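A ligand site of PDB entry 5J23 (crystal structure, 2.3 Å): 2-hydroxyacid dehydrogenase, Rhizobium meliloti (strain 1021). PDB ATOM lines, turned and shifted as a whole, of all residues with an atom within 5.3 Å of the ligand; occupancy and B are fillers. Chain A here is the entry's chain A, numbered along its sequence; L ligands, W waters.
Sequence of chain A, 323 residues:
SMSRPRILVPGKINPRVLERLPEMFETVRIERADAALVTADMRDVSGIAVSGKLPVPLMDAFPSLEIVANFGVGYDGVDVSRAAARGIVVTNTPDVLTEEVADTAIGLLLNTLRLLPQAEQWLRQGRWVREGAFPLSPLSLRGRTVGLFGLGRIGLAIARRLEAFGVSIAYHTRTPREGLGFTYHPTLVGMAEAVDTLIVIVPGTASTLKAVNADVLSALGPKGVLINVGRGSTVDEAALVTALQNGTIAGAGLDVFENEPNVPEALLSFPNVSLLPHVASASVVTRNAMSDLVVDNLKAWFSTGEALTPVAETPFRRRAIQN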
ATOM      1  N   VAL A  73     -36.747  -5.116  32.347  1.00  0.00           N
ATOM      2  CA  VAL A  73     -36.563  -5.304  30.913  1.00  0.00           C
ATOM      3  C   VAL A  73     -36.087  -6.718  30.636  1.00  0.00           C
ATOM      4  O   VAL A  73     -36.423  -7.295  29.593  1.00  0.00           O
ATOM      5  CB  VAL A  73     -35.676  -4.214  30.260  1.00  0.00           C
ATOM      6  CG1 VAL A  73     -34.222  -4.300  30.726  1.00  0.00           C
ATOM      7  CG2 VAL A  73     -35.766  -4.323  28.730  1.00  0.00           C
ATOM      8  N   GLY A  74     -35.280  -7.246  31.555  1.00  0.00           N
ATOM      9  CA  GLY A  74     -34.813  -8.609  31.500  1.00  0.00           C
ATOM     10  C   GLY A  74     -35.879  -9.550  32.000  1.00  0.00           C
ATOM     11  O   GLY A  74     -36.445  -9.286  33.039  1.00  0.00           O
ATOM     12  N   ASP A  76     -35.334 -13.133  31.805  1.00  0.00           N
ATOM     13  CA  ASP A  76     -34.685 -14.434  31.913  1.00  0.00           C
ATOM     14  C   ASP A  76     -35.138 -15.301  33.114  1.00  0.00           C
ATOM     15  O   ASP A  76     -34.914 -16.510  33.107  1.00  0.00           O
ATOM     16  CB  ASP A  76     -33.143 -14.270  31.862  1.00  0.00           C
ATOM     17  CG  ASP A  76     -32.615 -13.246  32.870  1.00  0.00           C
ATOM     18  OD1 ASP A  76     -32.845 -12.017  32.688  1.00  0.00           O
ATOM     19  OD2 ASP A  76     -32.003 -13.678  33.885  1.00  0.00           O
ATOM     20  N   THR A  98     -34.544   2.884  30.087  1.00  0.00           N
ATOM     21  CA  THR A  98     -33.370   2.923  29.212  1.00  0.00           C
ATOM     22  C   THR A  98     -32.348   4.004  29.616  1.00  0.00           C
ATOM     23  O   THR A  98     -31.156   3.729  29.681  1.00  0.00           O
ATOM     24  CB  THR A  98     -33.846   3.166  27.748  1.00  0.00           C
ATOM     25  OG1 THR A  98     -34.693   2.085  27.372  1.00  0.00           O
ATOM     26  CG2 THR A  98     -32.703   3.250  26.764  1.00  0.00           C
ATOM     27  N   VAL A 101     -30.670   3.331  33.153  1.00  0.00           N
ATOM     28  CA  VAL A 101     -29.679   2.261  33.129  1.00  0.00           C
ATOM     29  C   VAL A 101     -28.403   2.771  32.418  1.00  0.00           C
ATOM     30  O   VAL A 101     -27.278   2.449  32.817  1.00  0.00           O
ATOM     31  CB  VAL A 101     -30.238   1.015  32.412  1.00  0.00           C
ATOM     32  CG1 VAL A 101     -29.169  -0.007  32.151  1.00  0.00           C
ATOM     33  CG2 VAL A 101     -31.348   0.343  33.229  1.00  0.00           C
ATOM     34  N   PHE A 149     -20.773  -4.514  23.896  1.00  0.00           N
ATOM     35  CA  PHE A 149     -21.221  -5.864  23.615  1.00  0.00           C
ATOM     36  C   PHE A 149     -22.733  -5.830  23.807  1.00  0.00           C
ATOM     37  O   PHE A 149     -23.226  -5.764  24.940  1.00  0.00           O
ATOM     38  CB  PHE A 149     -20.558  -6.870  24.559  1.00  0.00           C
ATOM     39  CG  PHE A 149     -20.999  -8.295  24.370  1.00  0.00           C
ATOM     40  CD1 PHE A 149     -21.483  -8.763  23.150  1.00  0.00           C
ATOM     41  CD2 PHE A 149     -20.894  -9.194  25.422  1.00  0.00           C
ATOM     42  CE1 PHE A 149     -21.884 -10.079  22.986  1.00  0.00           C
ATOM     43  CE2 PHE A 149     -21.312 -10.510  25.273  1.00  0.00           C
ATOM     44  CZ  PHE A 149     -21.799 -10.953  24.048  1.00  0.00           C
ATOM     45  N   GLY A 150     -23.444  -5.805  22.684  1.00  0.00           N
ATOM     46  CA  GLY A 150     -24.878  -5.509  22.665  1.00  0.00           C
ATOM     47  C   GLY A 150     -25.071  -4.033  22.355  1.00  0.00           C
ATOM     48  O   GLY A 150     -24.262  -3.177  22.813  1.00  0.00           O
ATOM     49  N   LEU A 151     -26.120  -3.710  21.601  1.00  0.00           N
ATOM     50  CA  LEU A 151     -26.351  -2.335  21.157  1.00  0.00           C
ATOM     51  C   LEU A 151     -27.807  -2.050  20.861  1.00  0.00           C
ATOM     52  O   LEU A 151     -28.133  -1.453  19.833  1.00  0.00           O
ATOM     53  CB  LEU A 151     -25.494  -1.982  19.932  1.00  0.00           C
ATOM     54  CG  LEU A 151     -25.377  -0.457  19.674  1.00  0.00           C
ATOM     55  CD1 LEU A 151     -24.322   0.152  20.547  1.00  0.00           C
ATOM     56  CD2 LEU A 151     -25.082  -0.123  18.201  1.00  0.00           C
ATOM     57  N   GLY A 152     -28.683  -2.448  21.768  1.00  0.00           N
ATOM     58  CA  GLY A 152     -30.118  -2.236  21.565  1.00  0.00           C
ATOM     59  C   GLY A 152     -30.483  -0.842  22.051  1.00  0.00           C
ATOM     60  O   GLY A 152     -29.740   0.111  21.820  1.00  0.00           O
ATOM     61  N   ARG A 153     -31.593  -0.728  22.747  1.00  0.00           N
ATOM     62  CA  ARG A 153     -32.047   0.574  23.225  1.00  0.00           C
ATOM     63  C   ARG A 153     -31.042   1.147  24.248  1.00  0.00           C
ATOM     64  O   ARG A 153     -30.683   2.310  24.173  1.00  0.00           O
ATOM     65  CB  ARG A 153     -33.417   0.493  23.891  1.00  0.00           C
ATOM     66  CG  ARG A 153     -34.506  -0.376  23.220  1.00  0.00           C
ATOM     67  CD  ARG A 153     -35.436  -0.932  24.297  1.00  0.00           C
ATOM     68  NE  ARG A 153     -36.423  -1.873  23.800  1.00  0.00           N
ATOM     69  CZ  ARG A 153     -36.493  -3.183  24.098  1.00  0.00           C
ATOM     70  NH1 ARG A 153     -35.653  -3.776  24.956  1.00  0.00           N
ATOM     71  NH2 ARG A 153     -37.470  -3.897  23.554  1.00  0.00           N
ATOM     72  N   ILE A 154     -30.605   0.306  25.176  1.00  0.00           N
ATOM     73  CA  ILE A 154     -29.708   0.715  26.265  1.00  0.00           C
ATOM     74  C   ILE A 154     -28.284   0.931  25.742  1.00  0.00           C
ATOM     75  O   ILE A 154     -27.673   1.969  25.967  1.00  0.00           O
ATOM     76  CB  ILE A 154     -29.760  -0.265  27.448  1.00  0.00           C
ATOM     77  CG1 ILE A 154     -31.194  -0.333  28.011  1.00  0.00           C
ATOM     78  CG2 ILE A 154     -28.805   0.163  28.521  1.00  0.00           C
ATOM     79  CD1 ILE A 154     -31.452  -1.451  29.015  1.00  0.00           C
ATOM     80  N   GLY A 155     -27.780  -0.047  25.002  1.00  0.00           N
ATOM     81  CA  GLY A 155     -26.472   0.063  24.344  1.00  0.00           C
ATOM     82  C   GLY A 155     -26.344   1.339  23.521  1.00  0.00           C
ATOM     83  O   GLY A 155     -25.374   2.073  23.637  1.00  0.00           O
ATOM     84  N   HIS A 172     -20.338  -4.867  19.090  1.00  0.00           N
ATOM     85  CA  HIS A 172     -20.567  -6.222  18.626  1.00  0.00           C
ATOM     86  C   HIS A 172     -21.984  -6.714  18.927  1.00  0.00           C
ATOM     87  O   HIS A 172     -22.439  -6.695  20.080  1.00  0.00           O
ATOM     88  CB  HIS A 172     -19.612  -7.213  19.255  1.00  0.00           C
ATOM     89  CG  HIS A 172     -19.970  -8.622  18.948  1.00  0.00           C
ATOM     90  ND1 HIS A 172     -19.961  -9.125  17.656  1.00  0.00           N
ATOM     91  CD2 HIS A 172     -20.362  -9.647  19.746  1.00  0.00           C
ATOM     92  CE1 HIS A 172     -20.336 -10.393  17.686  1.00  0.00           C
ATOM     93  NE2 HIS A 172     -20.579 -10.728  18.943  1.00  0.00           N
ATOM     94  N   THR A 173     -22.624  -7.178  17.849  1.00  0.00           N
ATOM     95  CA  THR A 173     -23.983  -7.772  17.843  1.00  0.00           C
ATOM     96  C   THR A 173     -23.955  -8.895  16.827  1.00  0.00           C
ATOM     97  O   THR A 173     -23.041  -8.944  16.004  1.00  0.00           O
ATOM     98  CB  THR A 173     -25.080  -6.770  17.442  1.00  0.00           C
ATOM     99  OG1 THR A 173     -24.655  -6.004  16.299  1.00  0.00           O
ATOM    100  CG2 THR A 173     -25.400  -5.819  18.554  1.00  0.00           C
ATOM    101  N   ARG A 174     -24.968  -9.771  16.850  1.00  0.00           N
ATOM    102  CA  ARG A 174     -25.018 -10.914  15.917  1.00  0.00           C
ATOM    103  C   ARG A 174     -25.141 -10.417  14.492  1.00  0.00           C
ATOM    104  O   ARG A 174     -24.424 -10.887  13.598  1.00  0.00           O
ATOM    105  CB  ARG A 174     -26.161 -11.875  16.208  1.00  0.00           C
ATOM    106  CG  ARG A 174     -25.879 -12.831  17.362  1.00  0.00           C
ATOM    107  CD  ARG A 174     -27.143 -13.510  17.865  1.00  0.00           C
ATOM    108  NE  ARG A 174     -28.094 -12.558  18.446  1.00  0.00           N
ATOM    109  CZ  ARG A 174     -29.231 -12.897  19.068  1.00  0.00           C
ATOM    110  NH1 ARG A 174     -29.575 -14.170  19.218  1.00  0.00           N
ATOM    111  NH2 ARG A 174     -30.016 -11.926  19.558  1.00  0.00           N
ATOM    112  N   THR A 175     -26.053  -9.477  14.279  1.00  0.00           N
ATOM    113  CA  THR A 175     -26.164  -8.796  12.993  1.00  0.00           C
ATOM    114  C   THR A 175     -25.938  -7.287  13.199  1.00  0.00           C
ATOM    115  O   THR A 175     -26.390  -6.718  14.211  1.00  0.00           O
ATOM    116  CB  THR A 175     -27.497  -9.064  12.280  1.00  0.00           C
ATOM    117  OG1 THR A 175     -28.587  -8.587  13.071  1.00  0.00           O
ATOM    118  CG2 THR A 175     -27.673 -10.570  11.994  1.00  0.00           C
ATOM    119  N   ILE A 201     -23.801  -5.320  27.746  1.00  0.00           N
ATOM    120  CA  ILE A 201     -25.200  -4.854  27.830  1.00  0.00           C
ATOM    121  C   ILE A 201     -26.091  -5.705  26.921  1.00  0.00           C
ATOM    122  O   ILE A 201     -26.771  -5.211  26.008  1.00  0.00           O
ATOM    123  CB  ILE A 201     -25.290  -3.329  27.556  1.00  0.00           C
ATOM    124  CG1 ILE A 201     -26.717  -2.777  27.782  1.00  0.00           C
ATOM    125  CG2 ILE A 201     -24.809  -2.972  26.163  1.00  0.00           C
ATOM    126  CD1 ILE A 201     -27.345  -3.054  29.134  1.00  0.00           C
ATOM    127  N   VAL A 202     -26.057  -7.012  27.161  1.00  0.00           N
ATOM    128  CA  VAL A 202     -26.850  -7.961  26.381  1.00  0.00           C
ATOM    129  C   VAL A 202     -27.821  -8.665  27.301  1.00  0.00           C
ATOM    130  O   VAL A 202     -27.591  -8.690  28.528  1.00  0.00           O
ATOM    131  CB  VAL A 202     -25.983  -9.048  25.669  1.00  0.00           C
ATOM    132  CG1 VAL A 202     -25.141  -8.420  24.593  1.00  0.00           C
ATOM    133  CG2 VAL A 202     -25.112  -9.835  26.641  1.00  0.00           C
ATOM    134  N   PRO A 203     -28.891  -9.246  26.742  1.00  0.00           N
ATOM    135  CA  PRO A 203     -29.752 -10.125  27.557  1.00  0.00           C
ATOM    136  C   PRO A 203     -29.058 -11.393  28.091  1.00  0.00           C
ATOM    137  O   PRO A 203     -28.092 -11.894  27.488  1.00  0.00           O
ATOM    138  CB  PRO A 203     -30.905 -10.510  26.594  1.00  0.00           C
ATOM    139  CG  PRO A 203     -30.823  -9.532  25.452  1.00  0.00           C
ATOM    140  CD  PRO A 203     -29.380  -9.131  25.356  1.00  0.00           C
ATOM    141  N   GLY A 204     -29.576 -11.901  29.215  1.00  0.00           N
ATOM    142  CA  GLY A 204     -29.165 -13.183  29.804  1.00  0.00           C
ATOM    143  C   GLY A 204     -29.807 -14.366  29.109  1.00  0.00           C
ATOM    144  O   GLY A 204     -30.750 -14.980  29.633  1.00  0.00           O
ATOM    145  N   THR A 205     -29.281 -14.678  27.915  1.00  0.00           N
ATOM    146  CA  THR A 205     -29.731 -15.838  27.134  1.00  0.00           C
ATOM    147  C   THR A 205     -28.671 -16.939  27.110  1.00  0.00           C
ATOM    148  O   THR A 205     -27.524 -16.745  27.567  1.00  0.00           O
ATOM    149  CB  THR A 205     -30.118 -15.447  25.681  1.00  0.00           C
ATOM    150  OG1 THR A 205     -29.013 -14.817  25.001  1.00  0.00           O
ATOM    151  CG2 THR A 205     -31.346 -14.521  25.671  1.00  0.00           C
ATOM    152  N   SER A 207     -27.330 -17.984  24.381  1.00  0.00           N
ATOM    153  CA  SER A 207     -26.362 -17.542  23.371  1.00  0.00           C
ATOM    154  C   SER A 207     -25.202 -16.735  23.965  1.00  0.00           C
ATOM    155  O   SER A 207     -24.080 -16.832  23.476  1.00  0.00           O
ATOM    156  CB  SER A 207     -27.075 -16.718  22.292  1.00  0.00           C
ATOM    157  OG  SER A 207     -27.713 -15.590  22.869  1.00  0.00           O
ATOM    158  N   THR A 208     -25.486 -15.937  25.014  1.00  0.00           N
ATOM    159  CA  THR A 208     -24.484 -15.079  25.646  1.00  0.00           C
ATOM    160  C   THR A 208     -23.859 -15.685  26.917  1.00  0.00           C
ATOM    161  O   THR A 208     -22.988 -15.074  27.517  1.00  0.00           O
ATOM    162  CB  THR A 208     -25.061 -13.677  25.977  1.00  0.00           C
ATOM    163  OG1 THR A 208     -25.941 -13.754  27.105  1.00  0.00           O
ATOM    164  CG2 THR A 208     -25.815 -13.117  24.772  1.00  0.00           C
ATOM    165  N   VAL A 229     -23.194  -4.339  32.949  1.00  0.00           N
ATOM    166  CA  VAL A 229     -24.517  -3.884  33.353  1.00  0.00           C
ATOM    167  C   VAL A 229     -25.642  -4.714  32.657  1.00  0.00           C
ATOM    168  O   VAL A 229     -26.785  -4.276  32.575  1.00  0.00           O
ATOM    169  CB  VAL A 229     -24.734  -2.390  33.042  1.00  0.00           C
ATOM    170  CG1 VAL A 229     -23.993  -1.540  34.060  1.00  0.00           C
ATOM    171  CG2 VAL A 229     -24.325  -2.041  31.612  1.00  0.00           C
ATOM    172  N   GLY A 230     -25.308  -5.927  32.226  1.00  0.00           N
ATOM    173  CA  GLY A 230     -26.245  -6.774  31.503  1.00  0.00           C
ATOM    174  C   GLY A 230     -26.796  -7.833  32.448  1.00  0.00           C
ATOM    175  O   GLY A 230     -27.672  -7.545  33.257  1.00  0.00           O
ATOM    176  N   ARG A 231     -26.234  -9.023  32.354  1.00  0.00           N
ATOM    177  CA  ARG A 231     -26.546 -10.108  33.266  1.00  0.00           C
ATOM    178  C   ARG A 231     -25.247 -10.779  33.695  1.00  0.00           C
ATOM    179  O   ARG A 231     -24.303 -10.919  32.888  1.00  0.00           O
ATOM    180  CB  ARG A 231     -27.496 -11.139  32.618  1.00  0.00           C
ATOM    181  CG  ARG A 231     -28.959 -10.699  32.587  1.00  0.00           C
ATOM    182  CD  ARG A 231     -29.666 -10.894  33.923  1.00  0.00           C
ATOM    183  NE  ARG A 231     -30.994 -10.292  33.964  1.00  0.00           N
ATOM    184  CZ  ARG A 231     -31.248  -8.985  34.157  1.00  0.00           C
ATOM    185  NH1 ARG A 231     -30.269  -8.074  34.306  1.00  0.00           N
ATOM    186  NH2 ARG A 231     -32.502  -8.569  34.147  1.00  0.00           N
HETATM  187  O1  LIG L   1     -27.753  -9.801  18.432  1.00  0.00           O
HETATM  188  P1  LIG L   1     -28.725  -8.690  18.066  1.00  0.00           P
HETATM  189  O2  LIG L   1     -28.425  -8.109  16.691  1.00  0.00           O
HETATM  190  O3  LIG L   1     -30.151  -9.144  18.186  1.00  0.00           O
HETATM  191  O4  LIG L   1     -28.399  -7.522  19.138  1.00  0.00           O
HETATM  192  C1  LIG L   1     -28.929  -7.503  20.473  1.00  0.00           C
HETATM  193  C2  LIG L   1     -27.797  -7.849  21.431  1.00  0.00           C
HETATM  194  N1  LIG L   1     -27.588  -9.281  21.582  1.00  0.00           N
HETATM  195  C3  LIG L   1     -26.455  -9.995  21.243  1.00  0.00           C
HETATM  196  N2  LIG L   1     -25.320  -9.517  20.705  1.00  0.00           N
HETATM  197  C4  LIG L   1     -24.458 -10.505  20.453  1.00  0.00           C
HETATM  198  N3  LIG L   1     -24.602 -11.818  20.678  1.00  0.00           N
HETATM  199  C5  LIG L   1     -25.754 -12.266  21.212  1.00  0.00           C
HETATM  200  N4  LIG L   1     -25.911 -13.583  21.394  1.00  0.00           N
HETATM  201  C6  LIG L   1     -26.751 -11.320  21.523  1.00  0.00           C
HETATM  202  N5  LIG L   1     -28.027 -11.439  22.047  1.00  0.00           N
HETATM  203  C7  LIG L   1     -28.478 -10.211  22.060  1.00  0.00           C
HETATM  204  O5  LIG L   1     -28.186  -7.300  22.679  1.00  0.00           O
HETATM  205  C8  LIG L   1     -29.240  -6.081  20.923  1.00  0.00           C
HETATM  206  O6  LIG L   1     -28.328  -5.170  20.327  1.00  0.00           O
HETATM  207  C9  LIG L   1     -29.006  -6.125  22.434  1.00  0.00           C
HETATM  208  C10 LIG L   1     -30.255  -6.194  23.270  1.00  0.00           C
HETATM  209  O7  LIG L   1     -31.071  -5.041  22.975  1.00  0.00           O
HETATM  210  P2  LIG L   1     -32.571  -4.965  23.490  1.00  0.00           P
HETATM  211  O8  LIG L   1     -33.351  -6.190  23.161  1.00  0.00           O
HETATM  212  O9  LIG L   1     -33.275  -3.759  22.893  1.00  0.00           O
HETATM  213  O10 LIG L   1     -32.491  -4.784  25.077  1.00  0.00           O
HETATM  214  P3  LIG L   1     -32.012  -3.623  26.060  1.00  0.00           P
HETATM  215  O11 LIG L   1     -33.237  -2.831  26.459  1.00  0.00           O
HETATM  216  O12 LIG L   1     -31.009  -2.711  25.404  1.00  0.00           O
HETATM  217  O13 LIG L   1     -31.497  -4.427  27.348  1.00  0.00           O
HETATM  218  C11 LIG L   1     -30.540  -5.489  27.221  1.00  0.00           C
HETATM  219  C12 LIG L   1     -30.389  -6.169  28.567  1.00  0.00           C
HETATM  220  C13 LIG L   1     -31.647  -6.790  29.163  1.00  0.00           C
HETATM  221  O14 LIG L   1     -31.914  -8.098  28.679  1.00  0.00           O
HETATM  222  C14 LIG L   1     -31.338  -6.768  30.659  1.00  0.00           C
HETATM  223  O15 LIG L   1     -31.130  -8.071  31.182  1.00  0.00           O
HETATM  224  C15 LIG L   1     -30.043  -5.965  30.767  1.00  0.00           C
HETATM  225  O16 LIG L   1     -29.982  -5.208  29.562  1.00  0.00           O
HETATM  226  O17 LIG L   1     -30.103  -5.164  31.859  1.00  0.00           O
HETATM  227  O   HOH W   1     -28.271  -4.682  34.795  1.00  0.00           O
HETATM  228  O   HOH W   2     -35.243  -0.646  27.407  1.00  0.00           O
HETATM  229  O   HOH W   3     -31.789 -10.562  30.396  1.00  0.00           O
HETATM  230  O   HOH W   4     -34.454  -8.128  27.516  1.00  0.00           O
HETATM  231  O   HOH W   5     -35.581  -7.693  25.009  1.00  0.00           O
HETATM  232  O   HOH W   6     -28.773  -5.371  15.947  1.00  0.00           O
HETATM  233  O   HOH W   7     -21.985 -12.741  19.930  1.00  0.00           O
HETATM  234  O   HOH W   8     -31.093  -4.887  34.172  1.00  0.00           O
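The backbone NH of Gly 152 is in hydrogen-bond range of an oxygen (O6) of the ligand.
OG of Ser 207 lies within hydrogen-bond range of N4 of the ligand (3.1 Å).
O11 of the ligand is in salt-bridge range of NH1 of Arg 153 (3.0 Å).
O12 of the ligand lies within hydrogen-bond range of N of Ile 154 (3.1 Å).
An oxygen (O15) of the ligand sits close to the guanidinium group (NH1) of Arg 231, 3.2 Å away.
N of Leu 151 lies within hydrogen-bond range of O6 of the ligand (2.9 Å).
The backbone NH (N) of Arg 174 sits at hydrogen-bond distance from an oxygen (O1) of the ligand, at 3.2 Å.
The guanidinium group (NE) of Arg 174 lies within salt-bridge range of an oxygen (O1) of the ligand, at 2.8 Å.
The backbone NH (N) of Arg 153 lies within hydrogen-bond range of an oxygen (O12) of the ligand (3.4 Å).
NE of Arg 231 lies within salt-bridge range of OD1 of Asp 76.
O of His 172 lies within hydrogen-bond range of N of Gly 150 (2.9 Å).
O of Thr 205 lies within hydrogen-bond range of OG1 of Thr 208 (3.4 Å).
O of Pro 203 is in hydrogen-bond range of OG1 of Thr 208 (2.9 Å).
The side-chain hydroxyl of Thr 173 lies within hydrogen-bond range of the backbone carbonyl oxygen of Thr 175 (2.8 Å).
The backbone NH of Ile 201 lies within hydrogen-bond range of the backbone carbonyl oxygen of Phe 149.
The side-chain hydroxyl of Ser 207 is in hydrogen-bond range of the side-chain hydroxyl of Thr 205, 2.6 Å away.
O of Thr 175 sits close to O2 of the ligand (3.5 Å).
Val 73 touches the ligand.
Gly 74 touches the ligand.
Phe 149 touches the ligand.
Gly 150 touches the ligand.
Thr 173 touches the ligand.
Ile 201 touches the ligand.
Val 202 touches the ligand (O to C12, 3.8 Å).
CA of Pro 203 touches O14 of the ligand, at 3.2 Å.
Thr 208 touches the ligand.
Val 229 touches the ligand.
Gly 230 touches the ligand (O to O17, 3.7 Å).
Hydrophobic or aromatic side chains within 4 Å of the ligand: Val 73, Phe 149, Ile 154, Ile 201, Val 202 and Pro 203.
Water W3 lies within hydrogen-bond range of O15 of the ligand (2.7 Å), N of Gly 204 (2.8 Å) and OD1 of Asp 76 (2.9 Å).
Water W4 bridges O14 of the ligand (2.8 Å) and O of Val 73 (3.0 Å).
Water W6 bridges an oxygen (O2) of the ligand and the backbone carbonyl oxygen of Thr 175.
Water W7 bridges NE2 of His 172 (2.6 Å) and N3 of the ligand (2.9 Å).
Water W2 bridges OG1 of Thr 98 (2.8 Å) and O11 of the ligand (3.1 Å).
Water W1 lies within hydrogen-bond range of the backbone carbonyl oxygen of Val 229, the backbone carbonyl oxygen of Gly 230 and an oxygen (O17) of the ligand.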
